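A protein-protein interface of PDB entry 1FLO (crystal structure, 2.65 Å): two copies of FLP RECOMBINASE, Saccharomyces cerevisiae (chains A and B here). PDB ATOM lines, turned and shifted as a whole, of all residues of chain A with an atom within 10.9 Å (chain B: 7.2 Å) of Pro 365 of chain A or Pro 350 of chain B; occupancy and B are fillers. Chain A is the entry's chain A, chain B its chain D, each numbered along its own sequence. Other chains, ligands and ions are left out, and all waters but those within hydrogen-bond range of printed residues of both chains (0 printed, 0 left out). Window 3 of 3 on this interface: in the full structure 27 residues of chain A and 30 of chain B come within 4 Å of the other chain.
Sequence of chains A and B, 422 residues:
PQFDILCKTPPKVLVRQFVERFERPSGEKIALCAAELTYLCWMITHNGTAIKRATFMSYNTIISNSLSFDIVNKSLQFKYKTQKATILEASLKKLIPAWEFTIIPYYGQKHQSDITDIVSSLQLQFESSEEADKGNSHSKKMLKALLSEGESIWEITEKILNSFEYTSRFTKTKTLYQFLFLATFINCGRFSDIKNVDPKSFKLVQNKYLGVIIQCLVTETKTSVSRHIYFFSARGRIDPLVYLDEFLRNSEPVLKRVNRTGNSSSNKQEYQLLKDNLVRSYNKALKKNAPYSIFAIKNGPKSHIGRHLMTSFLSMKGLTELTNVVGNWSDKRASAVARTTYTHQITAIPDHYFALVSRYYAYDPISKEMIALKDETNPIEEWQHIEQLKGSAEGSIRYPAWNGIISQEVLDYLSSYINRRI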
ATOM      1  N   SER A 315      -3.501 -10.692 -38.559  1.00  0.00           N
ATOM      2  CA  SER A 315      -2.482 -11.707 -38.713  1.00  0.00           C
ATOM      3  C   SER A 315      -1.153 -11.138 -38.241  1.00  0.00           C
ATOM      4  O   SER A 315      -0.438 -11.768 -37.463  1.00  0.00           O
ATOM      5  CB  SER A 315      -2.355 -12.120 -40.170  1.00  0.00           C
ATOM      6  OG  SER A 315      -1.095 -12.744 -40.409  1.00  0.00           O
ATOM      7  N   MET A 316      -0.839  -9.939 -38.721  1.00  0.00           N
ATOM      8  CA  MET A 316       0.401  -9.267 -38.376  1.00  0.00           C
ATOM      9  C   MET A 316       0.520  -9.056 -36.861  1.00  0.00           C
ATOM     10  O   MET A 316       1.547  -9.369 -36.263  1.00  0.00           O
ATOM     11  CB  MET A 316       0.479  -7.924 -39.110  1.00  0.00           C
ATOM     12  CG  MET A 316       1.800  -7.178 -38.916  1.00  0.00           C
ATOM     13  SD  MET A 316       1.571  -5.491 -38.346  1.00  0.00           S
ATOM     14  CE  MET A 316       1.049  -5.834 -36.684  1.00  0.00           C
ATOM     15  N   LYS A 317      -0.540  -8.538 -36.256  1.00  0.00           N
ATOM     16  CA  LYS A 317      -0.599  -8.277 -34.821  1.00  0.00           C
ATOM     17  C   LYS A 317      -0.646  -9.550 -33.988  1.00  0.00           C
ATOM     18  O   LYS A 317      -0.872  -9.503 -32.778  1.00  0.00           O
ATOM     19  CB  LYS A 317      -1.839  -7.439 -34.493  1.00  0.00           C
ATOM     20  CG  LYS A 317      -1.701  -5.975 -34.806  1.00  0.00           C
ATOM     21  CD  LYS A 317      -0.765  -5.309 -33.796  1.00  0.00           C
ATOM     22  CE  LYS A 317      -0.519  -3.842 -34.146  1.00  0.00           C
ATOM     23  NZ  LYS A 317       0.247  -3.140 -33.081  1.00  0.00           N
ATOM     24  N   GLY A 318      -0.441 -10.692 -34.626  1.00  0.00           N
ATOM     25  CA  GLY A 318      -0.511 -11.946 -33.892  1.00  0.00           C
ATOM     26  C   GLY A 318      -1.813 -12.136 -33.114  1.00  0.00           C
ATOM     27  O   GLY A 318      -1.812 -12.633 -31.999  1.00  0.00           O
ATOM     28  N   LEU A 319      -2.935 -11.752 -33.710  1.00  0.00           N
ATOM     29  CA  LEU A 319      -4.222 -11.873 -33.049  1.00  0.00           C
ATOM     30  C   LEU A 319      -5.230 -12.671 -33.901  1.00  0.00           C
ATOM     31  O   LEU A 319      -6.425 -12.343 -33.968  1.00  0.00           O
ATOM     32  CB  LEU A 319      -4.757 -10.472 -32.764  1.00  0.00           C
ATOM     33  CG  LEU A 319      -3.966  -9.642 -31.744  1.00  0.00           C
ATOM     34  CD1 LEU A 319      -4.411  -8.173 -31.779  1.00  0.00           C
ATOM     35  CD2 LEU A 319      -4.177 -10.230 -30.346  1.00  0.00           C
ATOM     36  N   GLU A 321      -6.787 -15.076 -33.327  1.00  0.00           N
ATOM     37  CA  GLU A 321      -7.822 -15.761 -32.582  1.00  0.00           C
ATOM     38  C   GLU A 321      -9.106 -14.958 -32.659  1.00  0.00           C
ATOM     39  O   GLU A 321     -10.165 -15.428 -32.249  1.00  0.00           O
ATOM     40  CB  GLU A 321      -7.396 -15.943 -31.126  1.00  0.00           C
ATOM     41  CG  GLU A 321      -7.256 -14.648 -30.352  1.00  0.00           C
ATOM     42  CD  GLU A 321      -6.386 -14.819 -29.116  1.00  0.00           C
ATOM     43  OE1 GLU A 321      -5.148 -14.669 -29.227  1.00  0.00           O
ATOM     44  OE2 GLU A 321      -6.938 -15.120 -28.036  1.00  0.00           O
ATOM     45  N   LEU A 356      -8.384  -1.858 -29.354  1.00  0.00           N
ATOM     46  CA  LEU A 356      -7.277  -1.836 -30.302  1.00  0.00           C
ATOM     47  C   LEU A 356      -7.556  -0.943 -31.503  1.00  0.00           C
ATOM     48  O   LEU A 356      -6.822   0.002 -31.766  1.00  0.00           O
ATOM     49  CB  LEU A 356      -6.974  -3.266 -30.771  1.00  0.00           C
ATOM     50  CG  LEU A 356      -5.939  -3.466 -31.885  1.00  0.00           C
ATOM     51  CD1 LEU A 356      -4.557  -2.995 -31.414  1.00  0.00           C
ATOM     52  CD2 LEU A 356      -5.900  -4.943 -32.290  1.00  0.00           C
ATOM     53  N   TYR A 361      -5.961   2.690 -27.264  1.00  0.00           N
ATOM     54  CA  TYR A 361      -5.096   1.775 -26.546  1.00  0.00           C
ATOM     55  C   TYR A 361      -4.106   1.078 -27.467  1.00  0.00           C
ATOM     56  O   TYR A 361      -4.179   1.185 -28.687  1.00  0.00           O
ATOM     57  CB  TYR A 361      -5.921   0.710 -25.837  1.00  0.00           C
ATOM     58  CG  TYR A 361      -6.940   1.243 -24.871  1.00  0.00           C
ATOM     59  CD1 TYR A 361      -8.076   1.920 -25.316  1.00  0.00           C
ATOM     60  CD2 TYR A 361      -6.808   1.013 -23.508  1.00  0.00           C
ATOM     61  CE1 TYR A 361      -9.064   2.342 -24.419  1.00  0.00           C
ATOM     62  CE2 TYR A 361      -7.790   1.435 -22.602  1.00  0.00           C
ATOM     63  CZ  TYR A 361      -8.910   2.091 -23.063  1.00  0.00           C
ATOM     64  OH  TYR A 361      -9.878   2.470 -22.169  1.00  0.00           O
ATOM     65  N   ALA A 362      -3.164   0.367 -26.868  1.00  0.00           N
ATOM     66  CA  ALA A 362      -2.190  -0.387 -27.630  1.00  0.00           C
ATOM     67  C   ALA A 362      -2.189  -1.790 -27.047  1.00  0.00           C
ATOM     68  O   ALA A 362      -2.430  -1.976 -25.847  1.00  0.00           O
ATOM     69  CB  ALA A 362      -0.831   0.226 -27.501  1.00  0.00           C
ATOM     70  N   TYR A 363      -1.945  -2.776 -27.900  1.00  0.00           N
ATOM     71  CA  TYR A 363      -1.908  -4.164 -27.464  1.00  0.00           C
ATOM     72  C   TYR A 363      -0.500  -4.473 -26.995  1.00  0.00           C
ATOM     73  O   TYR A 363       0.459  -4.288 -27.748  1.00  0.00           O
ATOM     74  CB  TYR A 363      -2.265  -5.096 -28.628  1.00  0.00           C
ATOM     75  CG  TYR A 363      -2.151  -6.569 -28.319  1.00  0.00           C
ATOM     76  CD1 TYR A 363      -2.888  -7.146 -27.282  1.00  0.00           C
ATOM     77  CD2 TYR A 363      -1.318  -7.388 -29.073  1.00  0.00           C
ATOM     78  CE1 TYR A 363      -2.798  -8.513 -27.006  1.00  0.00           C
ATOM     79  CE2 TYR A 363      -1.217  -8.752 -28.809  1.00  0.00           C
ATOM     80  CZ  TYR A 363      -1.960  -9.309 -27.778  1.00  0.00           C
ATOM     81  OH  TYR A 363      -1.888 -10.663 -27.547  1.00  0.00           O
ATOM     82  N   ASP A 364      -0.371  -4.933 -25.755  1.00  0.00           N
ATOM     83  CA  ASP A 364       0.938  -5.280 -25.221  1.00  0.00           C
ATOM     84  C   ASP A 364       1.182  -6.781 -25.369  1.00  0.00           C
ATOM     85  O   ASP A 364       0.538  -7.592 -24.708  1.00  0.00           O
ATOM     86  CB  ASP A 364       1.035  -4.913 -23.748  1.00  0.00           C
ATOM     87  CG  ASP A 364       2.363  -5.325 -23.142  1.00  0.00           C
ATOM     88  OD1 ASP A 364       2.428  -5.449 -21.905  1.00  0.00           O
ATOM     89  OD2 ASP A 364       3.339  -5.516 -23.905  1.00  0.00           O
ATOM     90  N   PRO A 365       2.149  -7.167 -26.210  1.00  0.00           N
ATOM     91  CA  PRO A 365       2.448  -8.586 -26.421  1.00  0.00           C
ATOM     92  C   PRO A 365       2.724  -9.345 -25.131  1.00  0.00           C
ATOM     93  O   PRO A 365       1.964 -10.229 -24.742  1.00  0.00           O
ATOM     94  CB  PRO A 365       3.677  -8.549 -27.330  1.00  0.00           C
ATOM     95  CG  PRO A 365       3.553  -7.218 -28.037  1.00  0.00           C
ATOM     96  CD  PRO A 365       3.108  -6.314 -26.933  1.00  0.00           C
ATOM     97  N   ILE A 366       3.820  -8.985 -24.475  1.00  0.00           N
ATOM     98  CA  ILE A 366       4.259  -9.619 -23.234  1.00  0.00           C
ATOM     99  C   ILE A 366       3.135  -9.971 -22.248  1.00  0.00           C
ATOM    100  O   ILE A 366       2.957 -11.134 -21.886  1.00  0.00           O
ATOM    101  CB  ILE A 366       5.346  -8.734 -22.530  1.00  0.00           C
ATOM    102  CG1 ILE A 366       5.813  -9.401 -21.245  1.00  0.00           C
ATOM    103  CG2 ILE A 366       4.811  -7.354 -22.241  1.00  0.00           C
ATOM    104  CD1 ILE A 366       6.481 -10.723 -21.488  1.00  0.00           C
ATOM    105  N   SER A 367       2.368  -8.976 -21.829  1.00  0.00           N
ATOM    106  CA  SER A 367       1.286  -9.216 -20.883  1.00  0.00           C
ATOM    107  C   SER A 367      -0.035  -9.613 -21.541  1.00  0.00           C
ATOM    108  O   SER A 367      -0.892 -10.231 -20.899  1.00  0.00           O
ATOM    109  CB  SER A 367       1.060  -7.972 -20.026  1.00  0.00           C
ATOM    110  OG  SER A 367       0.742  -6.846 -20.827  1.00  0.00           O
ATOM    111  N   LYS A 368      -0.198  -9.253 -22.813  1.00  0.00           N
ATOM    112  CA  LYS A 368      -1.420  -9.558 -23.555  1.00  0.00           C
ATOM    113  C   LYS A 368      -2.580  -8.697 -23.052  1.00  0.00           C
ATOM    114  O   LYS A 368      -3.745  -9.110 -23.082  1.00  0.00           O
ATOM    115  CB  LYS A 368      -1.776 -11.046 -23.424  1.00  0.00           C
ATOM    116  CG  LYS A 368      -0.794 -11.990 -24.106  1.00  0.00           C
ATOM    117  CD  LYS A 368      -1.262 -13.429 -23.995  1.00  0.00           C
ATOM    118  CE  LYS A 368      -0.230 -14.399 -24.558  1.00  0.00           C
ATOM    119  NZ  LYS A 368      -0.638 -15.827 -24.370  1.00  0.00           N
ATOM    120  N   GLU A 369      -2.249  -7.498 -22.587  1.00  0.00           N
ATOM    121  CA  GLU A 369      -3.251  -6.570 -22.081  1.00  0.00           C
ATOM    122  C   GLU A 369      -3.243  -5.265 -22.877  1.00  0.00           C
ATOM    123  O   GLU A 369      -2.276  -4.944 -23.581  1.00  0.00           O
ATOM    124  CB  GLU A 369      -2.988  -6.263 -20.609  1.00  0.00           C
ATOM    125  CG  GLU A 369      -3.254  -7.408 -19.637  1.00  0.00           C
ATOM    126  CD  GLU A 369      -4.733  -7.661 -19.395  1.00  0.00           C
ATOM    127  OE1 GLU A 369      -5.479  -6.699 -19.115  1.00  0.00           O
ATOM    128  OE2 GLU A 369      -5.151  -8.831 -19.475  1.00  0.00           O
ATOM    129  N   MET A 370      -4.325  -4.510 -22.754  1.00  0.00           N
ATOM    130  CA  MET A 370      -4.445  -3.243 -23.459  1.00  0.00           C
ATOM    131  C   MET A 370      -3.964  -2.078 -22.581  1.00  0.00           C
ATOM    132  O   MET A 370      -4.432  -1.887 -21.442  1.00  0.00           O
ATOM    133  CB  MET A 370      -5.910  -3.016 -23.879  1.00  0.00           C
ATOM    134  CG  MET A 370      -6.482  -4.035 -24.902  1.00  0.00           C
ATOM    135  SD  MET A 370      -5.679  -4.031 -26.528  1.00  0.00           S
ATOM    136  CE  MET A 370      -5.958  -5.753 -27.051  1.00  0.00           C
ATOM    137  N   ILE A 371      -3.030  -1.297 -23.120  1.00  0.00           N
ATOM    138  CA  ILE A 371      -2.477  -0.149 -22.410  1.00  0.00           C
ATOM    139  C   ILE A 371      -2.957   1.175 -23.000  1.00  0.00           C
ATOM    140  O   ILE A 371      -2.692   1.479 -24.161  1.00  0.00           O
ATOM    141  CB  ILE A 371      -0.939  -0.132 -22.474  1.00  0.00           C
ATOM    142  CG1 ILE A 371      -0.364  -1.412 -21.878  1.00  0.00           C
ATOM    143  CG2 ILE A 371      -0.407   1.083 -21.726  1.00  0.00           C
ATOM    144  CD1 ILE A 371       1.121  -1.552 -22.133  1.00  0.00           C
ATOM    145  N   ASN B 207      13.967  -1.349 -32.379  1.00  0.00           N
ATOM    146  CA  ASN B 207      13.585  -2.153 -31.225  1.00  0.00           C
ATOM    147  C   ASN B 207      13.746  -1.292 -29.977  1.00  0.00           C
ATOM    148  O   ASN B 207      14.809  -0.709 -29.757  1.00  0.00           O
ATOM    149  CB  ASN B 207      14.484  -3.386 -31.122  1.00  0.00           C
ATOM    150  CG  ASN B 207      14.072  -4.321 -29.990  1.00  0.00           C
ATOM    151  OD1 ASN B 207      14.246  -4.008 -28.807  1.00  0.00           O
ATOM    152  ND2 ASN B 207      13.517  -5.477 -30.354  1.00  0.00           N
ATOM    153  N   TYR B 209      14.641  -1.749 -27.251  1.00  0.00           N
ATOM    154  CA  TYR B 209      15.562  -2.350 -26.294  1.00  0.00           C
ATOM    155  C   TYR B 209      17.014  -2.276 -26.770  1.00  0.00           C
ATOM    156  O   TYR B 209      17.902  -1.853 -26.032  1.00  0.00           O
ATOM    157  CB  TYR B 209      15.175  -3.816 -26.056  1.00  0.00           C
ATOM    158  CG  TYR B 209      13.845  -4.017 -25.352  1.00  0.00           C
ATOM    159  CD1 TYR B 209      12.947  -4.998 -25.781  1.00  0.00           C
ATOM    160  CD2 TYR B 209      13.503  -3.260 -24.230  1.00  0.00           C
ATOM    161  CE1 TYR B 209      11.747  -5.218 -25.110  1.00  0.00           C
ATOM    162  CE2 TYR B 209      12.305  -3.474 -23.553  1.00  0.00           C
ATOM    163  CZ  TYR B 209      11.433  -4.453 -23.996  1.00  0.00           C
ATOM    164  OH  TYR B 209      10.250  -4.660 -23.322  1.00  0.00           O
ATOM    165  N   GLU B 321       4.263 -19.732 -25.578  1.00  0.00           N
ATOM    166  CA  GLU B 321       3.412 -19.151 -26.607  1.00  0.00           C
ATOM    167  C   GLU B 321       4.298 -18.459 -27.644  1.00  0.00           C
ATOM    168  O   GLU B 321       4.108 -18.605 -28.850  1.00  0.00           O
ATOM    169  CB  GLU B 321       2.439 -18.127 -25.997  1.00  0.00           C
ATOM    170  CG  GLU B 321       1.659 -18.609 -24.762  1.00  0.00           C
ATOM    171  CD  GLU B 321       2.287 -18.148 -23.445  1.00  0.00           C
ATOM    172  OE1 GLU B 321       2.350 -16.919 -23.205  1.00  0.00           O
ATOM    173  OE2 GLU B 321       2.715 -19.014 -22.649  1.00  0.00           O
ATOM    174  N   LEU B 322       5.279 -17.713 -27.153  1.00  0.00           N
ATOM    175  CA  LEU B 322       6.205 -16.978 -27.998  1.00  0.00           C
ATOM    176  C   LEU B 322       6.901 -17.875 -29.013  1.00  0.00           C
ATOM    177  O   LEU B 322       7.425 -17.401 -30.015  1.00  0.00           O
ATOM    178  CB  LEU B 322       7.238 -16.278 -27.110  1.00  0.00           C
ATOM    179  CG  LEU B 322       8.233 -15.289 -27.724  1.00  0.00           C
ATOM    180  CD1 LEU B 322       7.560 -14.376 -28.744  1.00  0.00           C
ATOM    181  CD2 LEU B 322       8.835 -14.471 -26.598  1.00  0.00           C
ATOM    182  N   VAL B 325       5.328 -18.334 -32.847  1.00  0.00           N
ATOM    183  CA  VAL B 325       5.702 -17.240 -33.723  1.00  0.00           C
ATOM    184  C   VAL B 325       7.124 -17.392 -34.238  1.00  0.00           C
ATOM    185  O   VAL B 325       7.338 -17.513 -35.447  1.00  0.00           O
ATOM    186  CB  VAL B 325       5.565 -15.885 -33.003  1.00  0.00           C
ATOM    187  CG1 VAL B 325       5.869 -14.748 -33.951  1.00  0.00           C
ATOM    188  CG2 VAL B 325       4.173 -15.748 -32.449  1.00  0.00           C
ATOM    189  N   VAL B 326       8.082 -17.402 -33.310  1.00  0.00           N
ATOM    190  CA  VAL B 326       9.504 -17.510 -33.635  1.00  0.00           C
ATOM    191  C   VAL B 326       9.838 -18.681 -34.557  1.00  0.00           C
ATOM    192  O   VAL B 326      10.688 -18.557 -35.439  1.00  0.00           O
ATOM    193  CB  VAL B 326      10.354 -17.615 -32.349  1.00  0.00           C
ATOM    194  CG1 VAL B 326      11.827 -17.623 -32.700  1.00  0.00           C
ATOM    195  CG2 VAL B 326      10.053 -16.442 -31.429  1.00  0.00           C
ATOM    196  N   THR B 347       2.937 -12.649 -39.324  1.00  0.00           N
ATOM    197  CA  THR B 347       3.080 -12.221 -37.937  1.00  0.00           C
ATOM    198  C   THR B 347       4.520 -11.806 -37.665  1.00  0.00           C
ATOM    199  O   THR B 347       5.460 -12.442 -38.142  1.00  0.00           O
ATOM    200  CB  THR B 347       2.677 -13.348 -36.966  1.00  0.00           C
ATOM    201  OG1 THR B 347       1.335 -13.768 -37.255  1.00  0.00           O
ATOM    202  CG2 THR B 347       2.738 -12.857 -35.530  1.00  0.00           C
ATOM    203  N   ALA B 348       4.686 -10.725 -36.915  1.00  0.00           N
ATOM    204  CA  ALA B 348       6.019 -10.231 -36.583  1.00  0.00           C
ATOM    205  C   ALA B 348       6.418 -10.639 -35.169  1.00  0.00           C
ATOM    206  O   ALA B 348       5.583 -10.597 -34.254  1.00  0.00           O
ATOM    207  CB  ALA B 348       6.055  -8.709 -36.703  1.00  0.00           C
ATOM    208  N   ILE B 349       7.687 -11.031 -34.998  1.00  0.00           N
ATOM    209  CA  ILE B 349       8.234 -11.412 -33.684  1.00  0.00           C
ATOM    210  C   ILE B 349       8.138 -10.201 -32.726  1.00  0.00           C
ATOM    211  O   ILE B 349       8.498  -9.069 -33.086  1.00  0.00           O
ATOM    212  CB  ILE B 349       9.732 -11.809 -33.775  1.00  0.00           C
ATOM    213  CG1 ILE B 349       9.965 -12.870 -34.865  1.00  0.00           C
ATOM    214  CG2 ILE B 349      10.206 -12.292 -32.411  1.00  0.00           C
ATOM    215  CD1 ILE B 349       9.582 -14.281 -34.490  1.00  0.00           C
ATOM    216  N   PRO B 350       7.638 -10.422 -31.502  1.00  0.00           N
ATOM    217  CA  PRO B 350       7.504  -9.341 -30.513  1.00  0.00           C
ATOM    218  C   PRO B 350       8.847  -8.740 -30.090  1.00  0.00           C
ATOM    219  O   PRO B 350       9.840  -9.455 -29.924  1.00  0.00           O
ATOM    220  CB  PRO B 350       6.786 -10.021 -29.345  1.00  0.00           C
ATOM    221  CG  PRO B 350       5.993 -11.098 -30.020  1.00  0.00           C
ATOM    222  CD  PRO B 350       6.993 -11.651 -31.021  1.00  0.00           C
ATOM    223  N   ASP B 351       8.866  -7.425 -29.910  1.00  0.00           N
ATOM    224  CA  ASP B 351      10.086  -6.724 -29.532  1.00  0.00           C
ATOM    225  C   ASP B 351      10.773  -7.247 -28.275  1.00  0.00           C
ATOM    226  O   ASP B 351      12.002  -7.344 -28.239  1.00  0.00           O
ATOM    227  CB  ASP B 351       9.804  -5.226 -29.394  1.00  0.00           C
ATOM    228  CG  ASP B 351      10.133  -4.451 -30.668  1.00  0.00           C
ATOM    229  OD1 ASP B 351       9.968  -5.006 -31.778  1.00  0.00           O
ATOM    230  OD2 ASP B 351      10.554  -3.279 -30.559  1.00  0.00           O
ATOM    231  N   HIS B 352       9.995  -7.598 -27.254  1.00  0.00           N
ATOM    232  CA  HIS B 352      10.583  -8.092 -26.014  1.00  0.00           C
ATOM    233  C   HIS B 352      11.174  -9.495 -26.165  1.00  0.00           C
ATOM    234  O   HIS B 352      11.546 -10.131 -25.178  1.00  0.00           O
ATOM    235  CB  HIS B 352       9.548  -8.090 -24.886  1.00  0.00           C
ATOM    236  CG  HIS B 352       8.635  -9.272 -24.906  1.00  0.00           C
ATOM    237  ND1 HIS B 352       7.739  -9.500 -25.926  1.00  0.00           N
ATOM    238  CD2 HIS B 352       8.512 -10.317 -24.055  1.00  0.00           C
ATOM    239  CE1 HIS B 352       7.104 -10.638 -25.704  1.00  0.00           C
ATOM    240  NE2 HIS B 352       7.556 -11.154 -24.575  1.00  0.00           N
ATOM    241  N   TYR B 353      11.259  -9.985 -27.393  1.00  0.00           N
ATOM    242  CA  TYR B 353      11.823 -11.304 -27.604  1.00  0.00           C
ATOM    243  C   TYR B 353      13.327 -11.206 -27.590  1.00  0.00           C
ATOM    244  O   TYR B 353      13.993 -11.864 -26.804  1.00  0.00           O
ATOM    245  CB  TYR B 353      11.421 -11.885 -28.956  1.00  0.00           C
ATOM    246  CG  TYR B 353      12.296 -13.061 -29.349  1.00  0.00           C
ATOM    247  CD1 TYR B 353      12.167 -14.292 -28.705  1.00  0.00           C
ATOM    248  CD2 TYR B 353      13.260 -12.936 -30.350  1.00  0.00           C
ATOM    249  CE1 TYR B 353      12.968 -15.372 -29.051  1.00  0.00           C
ATOM    250  CE2 TYR B 353      14.066 -14.009 -30.706  1.00  0.00           C
ATOM    251  CZ  TYR B 353      13.913 -15.232 -30.052  1.00  0.00           C
ATOM    252  OH  TYR B 353      14.674 -16.330 -30.412  1.00  0.00           O
ATOM    253  N   PHE B 354      13.848 -10.391 -28.495  1.00  0.00           N
ATOM    254  CA  PHE B 354      15.278 -10.210 -28.633  1.00  0.00           C
ATOM    255  C   PHE B 354      15.927  -9.658 -27.372  1.00  0.00           C
ATOM    256  O   PHE B 354      17.099  -9.921 -27.104  1.00  0.00           O
ATOM    257  CB  PHE B 354      15.560  -9.301 -29.823  1.00  0.00           C
ATOM    258  CG  PHE B 354      14.872  -9.738 -31.084  1.00  0.00           C
ATOM    259  CD1 PHE B 354      13.527  -9.460 -31.285  1.00  0.00           C
ATOM    260  CD2 PHE B 354      15.565 -10.442 -32.063  1.00  0.00           C
ATOM    261  CE1 PHE B 354      12.881  -9.880 -32.444  1.00  0.00           C
ATOM    262  CE2 PHE B 354      14.930 -10.867 -33.225  1.00  0.00           C
ATOM    263  CZ  PHE B 354      13.587 -10.586 -33.420  1.00  0.00           C
ATOM    264  N   ALA B 355      15.164  -8.894 -26.599  1.00  0.00           N
ATOM    265  CA  ALA B 355      15.669  -8.336 -25.352  1.00  0.00           C
ATOM    266  C   ALA B 355      16.159  -9.475 -24.454  1.00  0.00           C
ATOM    267  O   ALA B 355      17.190  -9.365 -23.785  1.00  0.00           O
ATOM    268  CB  ALA B 355      14.571  -7.563 -24.648  1.00  0.00           C
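Among the printed residues, pairs that only touch across the chains: Ile 366 of chain A with His 352 of chain B (3.3 Å), Met 316 of chain A with Thr 347 of chain B (3.6 Å), Gly 318 of chain A with Thr 347 of chain B (3.8 Å) and Pro 365 of chain A with Pro 350 of chain B (3.99 Å).
OG1 of Thr 347 of chain B sits at hydrogen-bond distance from O of Ser 315 of chain A, at 2.7 Å. N of Ala 348 of chain B is in hydrogen-bond range of O of Met 316 of chain A, at 3.5 Å. OE1 of Glu 321 of chain B is in salt-bridge range of NZ of Lys 368 of chain A, 3.4 Å away.
Printed residues of chain A that touch a printed residue of chain B: Ser 315, Met 316, Gly 318, Pro 365, Ile 366 and Lys 368. Hydrophobic or aromatic side chains of chain A within 4 Å of the printed part of chain B: Pro 365 and Ile 366. Of the 15 printed residues of chain B, 5 touch a printed residue of chain A.
Printed residues of chain B within 4 Å of Ser 315 of chain A: Thr 347. Leu 356 of chain A touches none of the printed residues of chain B. Of the printed residues of chain B, Pro 365 of chain A touches Pro 350. Of the printed residues of chain B, Lys 368 of chain A touches Glu 321. Glu 369 of chain A touches none of the printed residues of chain B. Printed residues of chain A within 4 Å of Thr 347 of chain B: Ser 315, Met 316 and Gly 318. Ala 348 of chain B touches just one residue of chain A: Met 316 (3.5 Å). No residue of chain A comes within 4 Å of Ile 349 of chain B. Printed residues of chain A within 4 Å of Pro 350 of chain B: Pro 365. No residue of chain A comes within 4 Å of Asp 351 of chain B. His 352 of chain B touches just one residue of chain A: Ile 366. The nearest printed residue of chain A that does not touch Pro 350 of chain B is Ile 366 of chain A (5.8 Å).
1 position is printed for both chains. Of the 7 pairs that touch across the chains among the printed residues, none has its exchanged pair printed and touching as well.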
